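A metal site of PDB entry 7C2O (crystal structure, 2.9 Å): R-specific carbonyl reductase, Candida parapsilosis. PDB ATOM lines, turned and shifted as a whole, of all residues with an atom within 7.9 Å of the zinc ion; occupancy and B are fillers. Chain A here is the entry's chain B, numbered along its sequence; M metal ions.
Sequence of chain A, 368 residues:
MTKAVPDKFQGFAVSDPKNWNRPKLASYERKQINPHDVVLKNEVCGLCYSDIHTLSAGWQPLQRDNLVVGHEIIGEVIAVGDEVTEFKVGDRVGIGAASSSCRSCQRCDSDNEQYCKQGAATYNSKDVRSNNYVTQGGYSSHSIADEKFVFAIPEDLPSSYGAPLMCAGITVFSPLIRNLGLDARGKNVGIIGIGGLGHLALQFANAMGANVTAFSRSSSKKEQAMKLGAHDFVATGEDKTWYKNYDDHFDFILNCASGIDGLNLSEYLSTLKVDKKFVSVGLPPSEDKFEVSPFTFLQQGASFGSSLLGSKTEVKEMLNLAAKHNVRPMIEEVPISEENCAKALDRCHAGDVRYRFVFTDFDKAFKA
The side-chain sulfur (SG) of Cys 48 lies close to the backbone NH (N) of Ser 50 (3.4 Å).
The guanidinium group (NH2) of Arg 356 sits close to the side-chain sulfur (SG) of Cys 48, 3.6 Å away.
The backbone NH (N) of Cys 48 sits at hydrogen-bond distance from the side-chain carboxylate (OD2) of Asp 51 (3.1 Å).
O of Ser 50 sits at hydrogen-bond distance from OH of Tyr 123, 3.0 Å away.
OG of Ser 50 touches the zinc ion (3.7 Å).
Within 4 Å of the zinc ion: Cys 48, Ser 50, His 71 and Cys 167.
The zinc ion is bound by NE2 of His 71, SG of Cys 167 and SG of Cys 48.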
ATOM      1  N   GLY A  46      -4.497 -12.499 -11.076  1.00  0.00           N
ATOM      2  CA  GLY A  46      -4.141 -13.515 -10.114  1.00  0.00           C
ATOM      3  C   GLY A  46      -2.642 -13.687  -9.984  1.00  0.00           C
ATOM      4  O   GLY A  46      -1.874 -13.426 -10.908  1.00  0.00           O
ATOM      5  N   LEU A  47      -2.222 -14.129  -8.802  1.00  0.00           N
ATOM      6  CA  LEU A  47      -0.804 -14.354  -8.503  1.00  0.00           C
ATOM      7  C   LEU A  47      -0.446 -15.791  -8.873  1.00  0.00           C
ATOM      8  O   LEU A  47      -0.799 -16.722  -8.143  1.00  0.00           O
ATOM      9  CB  LEU A  47      -0.502 -14.070  -7.032  1.00  0.00           C
ATOM     10  CG  LEU A  47       0.932 -13.676  -6.660  1.00  0.00           C
ATOM     11  CD1 LEU A  47       0.957 -13.026  -5.291  1.00  0.00           C
ATOM     12  CD2 LEU A  47       1.881 -14.863  -6.693  1.00  0.00           C
ATOM     13  N   CYS A  48       0.257 -15.958  -9.974  1.00  0.00           N
ATOM     14  CA  CYS A  48       0.756 -17.261 -10.375  1.00  0.00           C
ATOM     15  C   CYS A  48       2.114 -17.527  -9.727  1.00  0.00           C
ATOM     16  O   CYS A  48       2.883 -16.613  -9.463  1.00  0.00           O
ATOM     17  CB  CYS A  48       0.886 -17.350 -11.901  1.00  0.00           C
ATOM     18  SG  CYS A  48       1.569 -18.910 -12.482  1.00  0.00           S
ATOM     19  N   TYR A  49       2.389 -18.807  -9.454  1.00  0.00           N
ATOM     20  CA  TYR A  49       3.643 -19.134  -8.777  1.00  0.00           C
ATOM     21  C   TYR A  49       4.839 -18.856  -9.675  1.00  0.00           C
ATOM     22  O   TYR A  49       5.924 -18.542  -9.174  1.00  0.00           O
ATOM     23  CB  TYR A  49       3.650 -20.586  -8.314  1.00  0.00           C
ATOM     24  CG  TYR A  49       4.676 -20.833  -7.233  1.00  0.00           C
ATOM     25  CD1 TYR A  49       4.356 -20.666  -5.902  1.00  0.00           C
ATOM     26  CD2 TYR A  49       5.976 -21.219  -7.556  1.00  0.00           C
ATOM     27  CE1 TYR A  49       5.293 -20.888  -4.903  1.00  0.00           C
ATOM     28  CE2 TYR A  49       6.921 -21.439  -6.570  1.00  0.00           C
ATOM     29  CZ  TYR A  49       6.572 -21.273  -5.248  1.00  0.00           C
ATOM     30  OH  TYR A  49       7.502 -21.496  -4.262  1.00  0.00           O
ATOM     31  N   SER A  50       4.674 -18.975 -10.992  1.00  0.00           N
ATOM     32  CA  SER A  50       5.757 -18.671 -11.921  1.00  0.00           C
ATOM     33  C   SER A  50       6.167 -17.211 -11.867  1.00  0.00           C
ATOM     34  O   SER A  50       7.230 -16.858 -12.387  1.00  0.00           O
ATOM     35  CB  SER A  50       5.343 -19.048 -13.347  1.00  0.00           C
ATOM     36  OG  SER A  50       4.700 -20.311 -13.382  1.00  0.00           O
ATOM     37  N   ASP A  51       5.336 -16.338 -11.282  1.00  0.00           N
ATOM     38  CA  ASP A  51       5.788 -14.986 -10.977  1.00  0.00           C
ATOM     39  C   ASP A  51       6.948 -15.012 -10.010  1.00  0.00           C
ATOM     40  O   ASP A  51       7.904 -14.232 -10.149  1.00  0.00           O
ATOM     41  CB  ASP A  51       4.634 -14.158 -10.400  1.00  0.00           C
ATOM     42  CG  ASP A  51       3.433 -14.075 -11.334  1.00  0.00           C
ATOM     43  OD1 ASP A  51       3.606 -14.278 -12.551  1.00  0.00           O
ATOM     44  OD2 ASP A  51       2.315 -13.797 -10.849  1.00  0.00           O
ATOM     45  N   GLY A  70       3.111 -11.232 -13.433  1.00  0.00           N
ATOM     46  CA  GLY A  70       1.681 -11.449 -13.356  1.00  0.00           C
ATOM     47  C   GLY A  70       1.073 -11.694 -14.715  1.00  0.00           C
ATOM     48  O   GLY A  70       1.103 -10.823 -15.588  1.00  0.00           O
ATOM     49  N   HIS A  71       0.517 -12.892 -14.922  1.00  0.00           N
ATOM     50  CA  HIS A  71      -0.039 -13.227 -16.228  1.00  0.00           C
ATOM     51  C   HIS A  71      -1.386 -13.917 -16.105  1.00  0.00           C
ATOM     52  O   HIS A  71      -1.734 -14.766 -16.938  1.00  0.00           O
ATOM     53  CB  HIS A  71       0.941 -14.092 -17.022  1.00  0.00           C
ATOM     54  CG  HIS A  71       1.402 -15.319 -16.299  1.00  0.00           C
ATOM     55  ND1 HIS A  71       2.658 -15.868 -16.487  1.00  0.00           N
ATOM     56  CD2 HIS A  71       0.785 -16.103 -15.384  1.00  0.00           C
ATOM     57  CE1 HIS A  71       2.777 -16.938 -15.725  1.00  0.00           C
ATOM     58  NE2 HIS A  71       1.659 -17.098 -15.047  1.00  0.00           N
ATOM     59  N   GLU A  72      -2.165 -13.570 -15.076  1.00  0.00           N
ATOM     60  CA  GLU A  72      -3.542 -14.030 -14.958  1.00  0.00           C
ATOM     61  C   GLU A  72      -4.464 -12.819 -15.022  1.00  0.00           C
ATOM     62  O   GLU A  72      -5.213 -12.541 -14.083  1.00  0.00           O
ATOM     63  CB  GLU A  72      -3.739 -14.804 -13.650  1.00  0.00           C
ATOM     64  CG  GLU A  72      -2.765 -15.966 -13.481  1.00  0.00           C
ATOM     65  CD  GLU A  72      -3.200 -16.964 -12.419  1.00  0.00           C
ATOM     66  OE1 GLU A  72      -3.880 -16.562 -11.448  1.00  0.00           O
ATOM     67  OE2 GLU A  72      -2.844 -18.164 -12.544  1.00  0.00           O
ATOM     68  N   GLY A  96      -3.479 -14.436 -20.764  1.00  0.00           N
ATOM     69  CA  GLY A  96      -2.793 -15.519 -20.086  1.00  0.00           C
ATOM     70  C   GLY A  96      -1.310 -15.278 -19.879  1.00  0.00           C
ATOM     71  O   GLY A  96      -0.888 -14.136 -19.635  1.00  0.00           O
ATOM     72  N   ALA A  97      -0.505 -16.344 -19.982  1.00  0.00           N
ATOM     73  CA  ALA A  97       0.934 -16.259 -19.746  1.00  0.00           C
ATOM     74  C   ALA A  97       1.744 -16.056 -21.026  1.00  0.00           C
ATOM     75  O   ALA A  97       2.961 -15.876 -20.945  1.00  0.00           O
ATOM     76  CB  ALA A  97       1.429 -17.515 -19.022  1.00  0.00           C
ATOM     77  N   TYR A 123       5.393 -11.670 -19.571  1.00  0.00           N
ATOM     78  CA  TYR A 123       6.401 -10.863 -18.903  1.00  0.00           C
ATOM     79  C   TYR A 123       7.774 -11.496 -19.090  1.00  0.00           C
ATOM     80  O   TYR A 123       7.891 -12.717 -19.278  1.00  0.00           O
ATOM     81  CB  TYR A 123       6.101 -10.677 -17.399  1.00  0.00           C
ATOM     82  CG  TYR A 123       5.929 -11.956 -16.606  1.00  0.00           C
ATOM     83  CD1 TYR A 123       7.026 -12.732 -16.248  1.00  0.00           C
ATOM     84  CD2 TYR A 123       4.668 -12.387 -16.207  1.00  0.00           C
ATOM     85  CE1 TYR A 123       6.870 -13.896 -15.522  1.00  0.00           C
ATOM     86  CE2 TYR A 123       4.504 -13.546 -15.477  1.00  0.00           C
ATOM     87  CZ  TYR A 123       5.613 -14.308 -15.134  1.00  0.00           C
ATOM     88  OH  TYR A 123       5.469 -15.463 -14.416  1.00  0.00           O
ATOM     89  N   PRO A 164      -7.689 -16.531 -12.227  1.00  0.00           N
ATOM     90  CA  PRO A 164      -6.833 -17.709 -12.082  1.00  0.00           C
ATOM     91  C   PRO A 164      -7.002 -18.737 -13.188  1.00  0.00           C
ATOM     92  O   PRO A 164      -6.107 -19.579 -13.374  1.00  0.00           O
ATOM     93  CB  PRO A 164      -7.243 -18.283 -10.718  1.00  0.00           C
ATOM     94  CG  PRO A 164      -7.830 -17.125  -9.991  1.00  0.00           C
ATOM     95  CD  PRO A 164      -8.538 -16.329 -11.035  1.00  0.00           C
ATOM     96  N   MET A 166      -6.974 -17.946 -16.321  1.00  0.00           N
ATOM     97  CA  MET A 166      -6.212 -17.477 -17.479  1.00  0.00           C
ATOM     98  C   MET A 166      -4.848 -18.148 -17.594  1.00  0.00           C
ATOM     99  O   MET A 166      -4.224 -18.060 -18.652  1.00  0.00           O
ATOM    100  CB  MET A 166      -6.044 -15.959 -17.406  1.00  0.00           C
ATOM    101  CG  MET A 166      -7.340 -15.188 -17.585  1.00  0.00           C
ATOM    102  SD  MET A 166      -8.096 -15.481 -19.198  1.00  0.00           S
ATOM    103  CE  MET A 166      -9.481 -16.512 -18.735  1.00  0.00           C
ATOM    104  N   CYS A 167      -4.372 -18.789 -16.537  1.00  0.00           N
ATOM    105  CA  CYS A 167      -3.105 -19.491 -16.590  1.00  0.00           C
ATOM    106  C   CYS A 167      -3.197 -20.807 -15.845  1.00  0.00           C
ATOM    107  O   CYS A 167      -3.068 -21.880 -16.446  1.00  0.00           O
ATOM    108  CB  CYS A 167      -1.983 -18.631 -15.996  1.00  0.00           C
ATOM    109  SG  CYS A 167      -0.413 -19.507 -15.897  1.00  0.00           S
ATOM    110  N   ALA A 168      -3.460 -20.747 -14.535  1.00  0.00           N
ATOM    111  CA  ALA A 168      -3.537 -21.961 -13.742  1.00  0.00           C
ATOM    112  C   ALA A 168      -4.602 -22.905 -14.279  1.00  0.00           C
ATOM    113  O   ALA A 168      -4.380 -24.119 -14.387  1.00  0.00           O
ATOM    114  CB  ALA A 168      -3.809 -21.617 -12.276  1.00  0.00           C
ATOM    115  N   ILE A 170      -6.021 -23.056 -17.448  1.00  0.00           N
ATOM    116  CA  ILE A 170      -5.673 -23.594 -18.753  1.00  0.00           C
ATOM    117  C   ILE A 170      -4.437 -24.486 -18.692  1.00  0.00           C
ATOM    118  O   ILE A 170      -4.273 -25.372 -19.546  1.00  0.00           O
ATOM    119  CB  ILE A 170      -5.490 -22.451 -19.781  1.00  0.00           C
ATOM    120  CG1 ILE A 170      -5.367 -23.001 -21.206  1.00  0.00           C
ATOM    121  CG2 ILE A 170      -4.273 -21.598 -19.438  1.00  0.00           C
ATOM    122  CD1 ILE A 170      -6.535 -23.872 -21.630  1.00  0.00           C
ATOM    123  N   THR A 171      -3.571 -24.299 -17.700  1.00  0.00           N
ATOM    124  CA  THR A 171      -2.358 -25.113 -17.617  1.00  0.00           C
ATOM    125  C   THR A 171      -2.681 -26.562 -17.251  1.00  0.00           C
ATOM    126  O   THR A 171      -1.941 -27.473 -17.631  1.00  0.00           O
ATOM    127  CB  THR A 171      -1.385 -24.511 -16.598  1.00  0.00           C
ATOM    128  OG1 THR A 171      -1.159 -23.129 -16.914  1.00  0.00           O
ATOM    129  CG2 THR A 171      -0.049 -25.242 -16.629  1.00  0.00           C
ATOM    130  N   LEU A 197      -2.617 -24.989  -8.737  1.00  0.00           N
ATOM    131  CA  LEU A 197      -2.880 -25.775  -9.943  1.00  0.00           C
ATOM    132  C   LEU A 197      -3.687 -27.017  -9.634  1.00  0.00           C
ATOM    133  O   LEU A 197      -4.623 -27.363 -10.373  1.00  0.00           O
ATOM    134  CB  LEU A 197      -1.559 -26.147 -10.617  1.00  0.00           C
ATOM    135  CG  LEU A 197      -0.790 -25.025 -11.305  1.00  0.00           C
ATOM    136  CD1 LEU A 197       0.656 -25.409 -11.457  1.00  0.00           C
ATOM    137  CD2 LEU A 197      -1.411 -24.713 -12.657  1.00  0.00           C
ATOM    138  N   GLY A 282       3.608 -26.796 -14.603  1.00  0.00           N
ATOM    139  CA  GLY A 282       4.016 -25.838 -13.587  1.00  0.00           C
ATOM    140  C   GLY A 282       5.408 -26.037 -13.043  1.00  0.00           C
ATOM    141  O   GLY A 282       5.759 -25.419 -12.031  1.00  0.00           O
ATOM    142  N   LEU A 308       2.697 -27.067 -21.516  1.00  0.00           N
ATOM    143  CA  LEU A 308       2.774 -25.627 -21.267  1.00  0.00           C
ATOM    144  C   LEU A 308       1.494 -24.966 -21.775  1.00  0.00           C
ATOM    145  O   LEU A 308       1.151 -25.115 -22.946  1.00  0.00           O
ATOM    146  CB  LEU A 308       3.993 -25.018 -21.941  1.00  0.00           C
ATOM    147  CG  LEU A 308       4.094 -23.489 -21.865  1.00  0.00           C
ATOM    148  CD1 LEU A 308       4.672 -23.050 -20.524  1.00  0.00           C
ATOM    149  CD2 LEU A 308       4.892 -22.907 -23.020  1.00  0.00           C
ATOM    150  N   LEU A 309       0.814 -24.251 -20.887  1.00  0.00           N
ATOM    151  CA  LEU A 309      -0.354 -23.413 -21.205  1.00  0.00           C
ATOM    152  C   LEU A 309      -1.402 -24.268 -21.928  1.00  0.00           C
ATOM    153  O   LEU A 309      -1.563 -25.462 -21.632  1.00  0.00           O
ATOM    154  CB  LEU A 309       0.103 -22.196 -21.976  1.00  0.00           C
ATOM    155  CG  LEU A 309       1.141 -21.367 -21.221  1.00  0.00           C
ATOM    156  CD1 LEU A 309       1.675 -20.234 -22.098  1.00  0.00           C
ATOM    157  CD2 LEU A 309       0.545 -20.847 -19.927  1.00  0.00           C
ATOM    158  N   ARG A 356      -5.616 -19.414  -4.288  1.00  0.00           N
ATOM    159  CA  ARG A 356      -5.030 -18.535  -5.291  1.00  0.00           C
ATOM    160  C   ARG A 356      -5.205 -17.087  -4.860  1.00  0.00           C
ATOM    161  O   ARG A 356      -6.333 -16.643  -4.625  1.00  0.00           O
ATOM    162  CB  ARG A 356      -5.684 -18.764  -6.659  1.00  0.00           C
ATOM    163  CG  ARG A 356      -4.719 -19.287  -7.700  1.00  0.00           C
ATOM    164  CD  ARG A 356      -3.591 -18.296  -7.965  1.00  0.00           C
ATOM    165  NE  ARG A 356      -2.953 -18.549  -9.257  1.00  0.00           N
ATOM    166  CZ  ARG A 356      -2.015 -19.466  -9.453  1.00  0.00           C
ATOM    167  NH1 ARG A 356      -1.596 -20.217  -8.444  1.00  0.00           N
ATOM    168  NH2 ARG A 356      -1.498 -19.625 -10.665  1.00  0.00           N
HETATM  169 ZN    ZN M   1       1.535 -19.077 -14.814  1.00  0.00          ZN
